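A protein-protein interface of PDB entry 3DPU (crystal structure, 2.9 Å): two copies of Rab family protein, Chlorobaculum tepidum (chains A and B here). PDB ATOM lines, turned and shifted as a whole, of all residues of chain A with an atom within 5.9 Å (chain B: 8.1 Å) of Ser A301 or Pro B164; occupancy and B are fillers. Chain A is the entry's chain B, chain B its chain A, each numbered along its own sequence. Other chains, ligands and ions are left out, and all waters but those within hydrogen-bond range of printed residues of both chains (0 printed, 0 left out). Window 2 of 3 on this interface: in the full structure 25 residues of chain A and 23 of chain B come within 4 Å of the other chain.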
ATOM      1  N   ASN A 299      -5.045 -13.937 -18.953  1.00  0.00           N
ATOM      2  CA  ASN A 299      -5.310 -12.547 -18.624  1.00  0.00           C
ATOM      3  C   ASN A 299      -4.105 -11.796 -18.103  1.00  0.00           C
ATOM      4  O   ASN A 299      -4.239 -10.724 -17.506  1.00  0.00           O
ATOM      5  CB  ASN A 299      -6.487 -12.441 -17.654  1.00  0.00           C
ATOM      6  CG  ASN A 299      -7.731 -11.865 -18.310  1.00  0.00           C
ATOM      7  OD1 ASN A 299      -8.721 -11.592 -17.627  1.00  0.00           O
ATOM      8  ND2 ASN A 299      -7.683 -11.652 -19.639  1.00  0.00           N
ATOM      9  N   SER A 300      -2.924 -12.356 -18.341  1.00  0.00           N
ATOM     10  CA  SER A 300      -1.672 -11.717 -17.943  1.00  0.00           C
ATOM     11  C   SER A 300      -1.358 -10.549 -18.869  1.00  0.00           C
ATOM     12  O   SER A 300      -1.742 -10.565 -20.043  1.00  0.00           O
ATOM     13  CB  SER A 300      -0.545 -12.737 -18.018  1.00  0.00           C
ATOM     14  OG  SER A 300       0.651 -12.207 -17.507  1.00  0.00           O
ATOM     15  N   SER A 301      -0.662  -9.539 -18.352  1.00  0.00           N
ATOM     16  CA  SER A 301      -0.103  -8.484 -19.208  1.00  0.00           C
ATOM     17  C   SER A 301       1.067  -8.998 -20.067  1.00  0.00           C
ATOM     18  O   SER A 301       1.358  -8.464 -21.133  1.00  0.00           O
ATOM     19  CB  SER A 301       0.353  -7.305 -18.365  1.00  0.00           C
ATOM     20  OG  SER A 301       1.420  -7.695 -17.526  1.00  0.00           O
ATOM     21  N   LYS A 302       1.730 -10.047 -19.583  1.00  0.00           N
ATOM     22  CA  LYS A 302       2.782 -10.742 -20.334  1.00  0.00           C
ATOM     23  C   LYS A 302       2.269 -11.601 -21.496  1.00  0.00           C
ATOM     24  O   LYS A 302       3.080 -12.094 -22.286  1.00  0.00           O
ATOM     25  CB  LYS A 302       3.652 -11.577 -19.397  1.00  0.00           C
ATOM     26  CG  LYS A 302       4.370 -10.750 -18.332  1.00  0.00           C
ATOM     27  CD  LYS A 302       5.731 -10.247 -18.787  1.00  0.00           C
ATOM     28  CE  LYS A 302       6.485  -9.591 -17.627  1.00  0.00           C
ATOM     29  NZ  LYS A 302       6.134  -8.149 -17.480  1.00  0.00           N
ATOM     30  N   THR A 303       0.945 -11.783 -21.602  1.00  0.00           N
ATOM     31  CA  THR A 303       0.344 -12.467 -22.767  1.00  0.00           C
ATOM     32  C   THR A 303      -0.619 -11.557 -23.548  1.00  0.00           C
ATOM     33  O   THR A 303      -1.412 -12.027 -24.375  1.00  0.00           O
ATOM     34  CB  THR A 303      -0.334 -13.793 -22.392  1.00  0.00           C
ATOM     35  OG1 THR A 303      -1.439 -13.530 -21.532  1.00  0.00           O
ATOM     36  CG2 THR A 303       0.628 -14.708 -21.665  1.00  0.00           C
ATOM     37  N   LYS A 304      -0.518 -10.253 -23.266  1.00  0.00           N
ATOM     38  CA  LYS A 304      -1.183  -9.162 -24.001  1.00  0.00           C
ATOM     39  C   LYS A 304      -1.404  -9.451 -25.492  1.00  0.00           C
ATOM     40  O   LYS A 304      -2.490  -9.198 -26.022  1.00  0.00           O
ATOM     41  CB  LYS A 304      -0.352  -7.869 -23.887  1.00  0.00           C
ATOM     42  CG  LYS A 304      -0.711  -6.904 -22.768  1.00  0.00           C
ATOM     43  CD  LYS A 304       0.319  -5.760 -22.673  1.00  0.00           C
ATOM     44  N   ASN A 305      -0.369  -9.964 -26.161  1.00  0.00           N
ATOM     45  CA  ASN A 305      -0.394 -10.106 -27.621  1.00  0.00           C
ATOM     46  C   ASN A 305      -0.310 -11.537 -28.157  1.00  0.00           C
ATOM     47  O   ASN A 305       0.105 -11.737 -29.297  1.00  0.00           O
ATOM     48  CB  ASN A 305       0.701  -9.251 -28.255  1.00  0.00           C
ATOM     49  CG  ASN A 305       0.696  -7.837 -27.744  1.00  0.00           C
ATOM     50  OD1 ASN A 305       0.119  -6.944 -28.363  1.00  0.00           O
ATOM     51  ND2 ASN A 305       1.328  -7.619 -26.599  1.00  0.00           N
ATOM     52  N   TYR A 315       6.697 -16.244 -13.022  1.00  0.00           N
ATOM     53  CA  TYR A 315       6.261 -14.892 -12.653  1.00  0.00           C
ATOM     54  C   TYR A 315       4.766 -14.679 -12.881  1.00  0.00           C
ATOM     55  O   TYR A 315       4.083 -14.106 -12.029  1.00  0.00           O
ATOM     56  CB  TYR A 315       7.060 -13.811 -13.401  1.00  0.00           C
ATOM     57  CG  TYR A 315       6.427 -12.446 -13.285  1.00  0.00           C
ATOM     58  CD1 TYR A 315       6.621 -11.657 -12.153  1.00  0.00           C
ATOM     59  CD2 TYR A 315       5.603 -11.958 -14.292  1.00  0.00           C
ATOM     60  CE1 TYR A 315       6.023 -10.401 -12.039  1.00  0.00           C
ATOM     61  CE2 TYR A 315       5.001 -10.711 -14.187  1.00  0.00           C
ATOM     62  CZ  TYR A 315       5.212  -9.945 -13.063  1.00  0.00           C
ATOM     63  OH  TYR A 315       4.619  -8.716 -12.976  1.00  0.00           O
ATOM     64  N   GLU A 320       2.534 -11.896 -10.193  1.00  0.00           N
ATOM     65  CA  GLU A 320       2.010 -10.757 -10.956  1.00  0.00           C
ATOM     66  C   GLU A 320       0.757 -10.108 -10.349  1.00  0.00           C
ATOM     67  O   GLU A 320      -0.230 -10.781 -10.055  1.00  0.00           O
ATOM     68  CB  GLU A 320       1.781 -11.136 -12.414  1.00  0.00           C
ATOM     69  CG  GLU A 320       1.584  -9.937 -13.335  1.00  0.00           C
ATOM     70  CD  GLU A 320       0.927 -10.303 -14.668  1.00  0.00           C
ATOM     71  OE1 GLU A 320       0.735 -11.513 -14.944  1.00  0.00           O
ATOM     72  OE2 GLU A 320       0.611  -9.367 -15.439  1.00  0.00           O
ATOM     73  N   SER B 131     -14.316  -5.049 -22.699  1.00  0.00           N
ATOM     74  CA  SER B 131     -14.354  -6.487 -22.956  1.00  0.00           C
ATOM     75  C   SER B 131     -15.781  -7.062 -22.917  1.00  0.00           C
ATOM     76  O   SER B 131     -16.248  -7.681 -23.870  1.00  0.00           O
ATOM     77  CB  SER B 131     -13.470  -7.179 -21.921  1.00  0.00           C
ATOM     78  OG  SER B 131     -13.219  -8.520 -22.265  1.00  0.00           O
ATOM     79  N   LYS B 159     -11.488  -0.329 -18.788  1.00  0.00           N
ATOM     80  CA  LYS B 159     -11.327  -1.457 -17.864  1.00  0.00           C
ATOM     81  C   LYS B 159     -10.163  -2.381 -18.275  1.00  0.00           C
ATOM     82  O   LYS B 159     -10.102  -3.547 -17.865  1.00  0.00           O
ATOM     83  CB  LYS B 159     -12.654  -2.231 -17.714  1.00  0.00           C
ATOM     84  N   ILE B 160      -9.237  -1.829 -19.064  1.00  0.00           N
ATOM     85  CA  ILE B 160      -8.067  -2.533 -19.612  1.00  0.00           C
ATOM     86  C   ILE B 160      -7.233  -3.302 -18.591  1.00  0.00           C
ATOM     87  O   ILE B 160      -6.572  -4.275 -18.936  1.00  0.00           O
ATOM     88  CB  ILE B 160      -7.192  -1.563 -20.458  1.00  0.00           C
ATOM     89  CG1 ILE B 160      -7.452  -1.777 -21.956  1.00  0.00           C
ATOM     90  CG2 ILE B 160      -5.714  -1.748 -20.196  1.00  0.00           C
ATOM     91  CD1 ILE B 160      -8.886  -1.592 -22.400  1.00  0.00           C
ATOM     92  N   ASP B 161      -7.282  -2.853 -17.339  1.00  0.00           N
ATOM     93  CA  ASP B 161      -6.584  -3.484 -16.217  1.00  0.00           C
ATOM     94  C   ASP B 161      -7.017  -4.940 -15.964  1.00  0.00           C
ATOM     95  O   ASP B 161      -6.211  -5.769 -15.536  1.00  0.00           O
ATOM     96  CB  ASP B 161      -6.775  -2.642 -14.947  1.00  0.00           C
ATOM     97  CG  ASP B 161      -8.242  -2.295 -14.675  1.00  0.00           C
ATOM     98  OD1 ASP B 161      -8.862  -2.947 -13.803  1.00  0.00           O
ATOM     99  OD2 ASP B 161      -8.777  -1.372 -15.329  1.00  0.00           O
ATOM    100  N   GLU B 162      -8.289  -5.235 -16.230  1.00  0.00           N
ATOM    101  CA  GLU B 162      -8.835  -6.579 -16.061  1.00  0.00           C
ATOM    102  C   GLU B 162      -8.523  -7.495 -17.250  1.00  0.00           C
ATOM    103  O   GLU B 162      -8.432  -8.716 -17.076  1.00  0.00           O
ATOM    104  CB  GLU B 162     -10.350  -6.523 -15.856  1.00  0.00           C
ATOM    105  CG  GLU B 162     -10.815  -5.767 -14.621  1.00  0.00           C
ATOM    106  CD  GLU B 162     -12.223  -5.189 -14.783  1.00  0.00           C
ATOM    107  OE1 GLU B 162     -13.047  -5.792 -15.517  1.00  0.00           O
ATOM    108  OE2 GLU B 162     -12.507  -4.128 -14.174  1.00  0.00           O
ATOM    109  N   ASN B 163      -8.391  -6.929 -18.452  1.00  0.00           N
ATOM    110  CA  ASN B 163      -8.079  -7.720 -19.655  1.00  0.00           C
ATOM    111  C   ASN B 163      -7.065  -7.028 -20.548  1.00  0.00           C
ATOM    112  O   ASN B 163      -7.445  -6.375 -21.526  1.00  0.00           O
ATOM    113  CB  ASN B 163      -9.345  -8.022 -20.460  1.00  0.00           C
ATOM    114  CG  ASN B 163     -10.528  -8.319 -19.580  1.00  0.00           C
ATOM    115  OD1 ASN B 163     -11.443  -7.503 -19.463  1.00  0.00           O
ATOM    116  ND2 ASN B 163     -10.503  -9.477 -18.917  1.00  0.00           N
ATOM    117  N   PRO B 164      -5.767  -7.168 -20.217  1.00  0.00           N
ATOM    118  CA  PRO B 164      -4.685  -6.508 -20.958  1.00  0.00           C
ATOM    119  C   PRO B 164      -4.725  -6.754 -22.471  1.00  0.00           C
ATOM    120  O   PRO B 164      -4.342  -5.881 -23.244  1.00  0.00           O
ATOM    121  CB  PRO B 164      -3.421  -7.116 -20.345  1.00  0.00           C
ATOM    122  CG  PRO B 164      -3.823  -7.559 -19.002  1.00  0.00           C
ATOM    123  CD  PRO B 164      -5.249  -7.969 -19.093  1.00  0.00           C
ATOM    124  N   SER B 165      -5.215  -7.917 -22.882  1.00  0.00           N
ATOM    125  CA  SER B 165      -5.239  -8.285 -24.293  1.00  0.00           C
ATOM    126  C   SER B 165      -6.332  -7.585 -25.101  1.00  0.00           C
ATOM    127  O   SER B 165      -6.356  -7.701 -26.326  1.00  0.00           O
ATOM    128  CB  SER B 165      -5.395  -9.798 -24.446  1.00  0.00           C
ATOM    129  OG  SER B 165      -6.729 -10.172 -24.190  1.00  0.00           O
ATOM    130  N   TYR B 166      -7.220  -6.852 -24.435  1.00  0.00           N
ATOM    131  CA  TYR B 166      -8.404  -6.307 -25.114  1.00  0.00           C
ATOM    132  C   TYR B 166      -8.171  -5.169 -26.121  1.00  0.00           C
ATOM    133  O   TYR B 166      -7.777  -4.061 -25.752  1.00  0.00           O
ATOM    134  CB  TYR B 166      -9.478  -5.907 -24.112  1.00  0.00           C
ATOM    135  CG  TYR B 166     -10.733  -5.420 -24.780  1.00  0.00           C
ATOM    136  CD1 TYR B 166     -11.186  -4.115 -24.584  1.00  0.00           C
ATOM    137  CD2 TYR B 166     -11.456  -6.249 -25.629  1.00  0.00           C
ATOM    138  CE1 TYR B 166     -12.336  -3.654 -25.210  1.00  0.00           C
ATOM    139  CE2 TYR B 166     -12.613  -5.795 -26.260  1.00  0.00           C
ATOM    140  CZ  TYR B 166     -13.042  -4.502 -26.041  1.00  0.00           C
ATOM    141  OH  TYR B 166     -14.174  -4.049 -26.646  1.00  0.00           O
ATOM    142  N   ASN B 167      -8.439  -5.455 -27.392  1.00  0.00           N
ATOM    143  CA  ASN B 167      -8.330  -4.454 -28.440  1.00  0.00           C
ATOM    144  C   ASN B 167      -9.386  -4.680 -29.508  1.00  0.00           C
ATOM    145  O   ASN B 167     -10.182  -5.602 -29.401  1.00  0.00           O
ATOM    146  CB  ASN B 167      -6.925  -4.459 -29.048  1.00  0.00           C
ATOM    147  CG  ASN B 167      -6.361  -3.056 -29.234  1.00  0.00           C
ATOM    148  OD1 ASN B 167      -5.246  -2.772 -28.789  1.00  0.00           O
ATOM    149  ND2 ASN B 167      -7.130  -2.166 -29.871  1.00  0.00           N
ATOM    150  N   ARG B 186      -6.693   3.143 -25.100  1.00  0.00           N
ATOM    151  CA  ARG B 186      -6.752   2.040 -24.154  1.00  0.00           C
ATOM    152  C   ARG B 186      -6.467   2.559 -22.740  1.00  0.00           C
ATOM    153  O   ARG B 186      -5.383   3.064 -22.461  1.00  0.00           O
ATOM    154  CB  ARG B 186      -5.791   0.934 -24.579  1.00  0.00           C
ATOM    155  CG  ARG B 186      -6.227   0.194 -25.844  1.00  0.00           C
ATOM    156  CD  ARG B 186      -5.279  -0.935 -26.181  1.00  0.00           C
ATOM    157  NE  ARG B 186      -4.673  -1.491 -24.974  1.00  0.00           N
ATOM    158  CZ  ARG B 186      -4.818  -2.748 -24.553  1.00  0.00           C
ATOM    159  NH1 ARG B 186      -5.530  -3.621 -25.259  1.00  0.00           N
ATOM    160  NH2 ARG B 186      -4.224  -3.141 -23.428  1.00  0.00           N
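The backbone carbonyl oxygen of Glu B162 sits close to the side-chain amide oxygen of Asn A299, at 2.9 Å.
OD1 of Asn A299 is in hydrogen-bond range of ND2 of Asn B163 (3.1 Å).
The side-chain hydroxyl of Ser B131 sits close to the side-chain amide oxygen of Asn B163, at 3.5 Å.
NH2 of Arg B186 lies within hydrogen-bond range of O of Pro B164 (2.7 Å).
The backbone NH (N) of Lys A302 sits at hydrogen-bond distance from the side-chain hydroxyl (OG) of Ser A300, at 3.2 Å.
The backbone carbonyl oxygen (O) of Ser A300 sits at hydrogen-bond distance from the side-chain hydroxyl (OG1) of Thr A303 (3.3 Å).
The side-chain carboxylate (OE1) of Glu A320 lies within hydrogen-bond range of the side-chain hydroxyl (OG) of Ser A300, 2.7 Å away.
The side-chain hydroxyl (OG) of Ser A301 lies within hydrogen-bond range of the side-chain carboxylate (OE2) of Glu A320 (2.8 Å).
Pro B164 touches Asn A299 (CD to O, 3.3 Å).
Ser A300 touches Pro B164.
CB of Pro B164 touches CA of Ser A301, 3.8 Å away.
Pro B164 touches Lys A304.
CB of Ser B165 touches O of Lys A304, at 3.4 Å.
Of the printed residues of chain B, Asn A299 touches Glu B162 (2.9 Å), Asn B163 (3.1 Å) and Pro B164 (3.3 Å).
Ser A301 touches just one residue of chain B: Pro B164.
Printed residues of chain B within 4 Å of Lys A304: Pro B164 (3.6 Å) and Ser B165 (3.4 Å).
Of the printed residues of chain A, Asn B163 touches Asn A299 (3.1 Å).
Pro B164 touches just these residues of chain A: Asn A299, Ser A300, Ser A301 and Lys A304.
Of the printed residues of chain A, Ser B165 touches Lys A304 (3.4 Å).
Arg B186 touches none of the printed residues of chain A.
Along chain A the printed residues that touch a printed residue of chain B span positions 299 to 304.
Hydrophobic or aromatic side chains of chain B that line the printed part of chain A: Pro B164.
Among the printed residues, 7 pairs touch across the chains.
Among the printed residues, no Asp or Glu carboxylate lies within 4 Å of a Lys or Arg side-chain nitrogen of the other chain.
No position is printed for both chains.
Of the 7 pairs that touch across the chains among the printed residues, none has its exchanged pair printed and touching as well.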
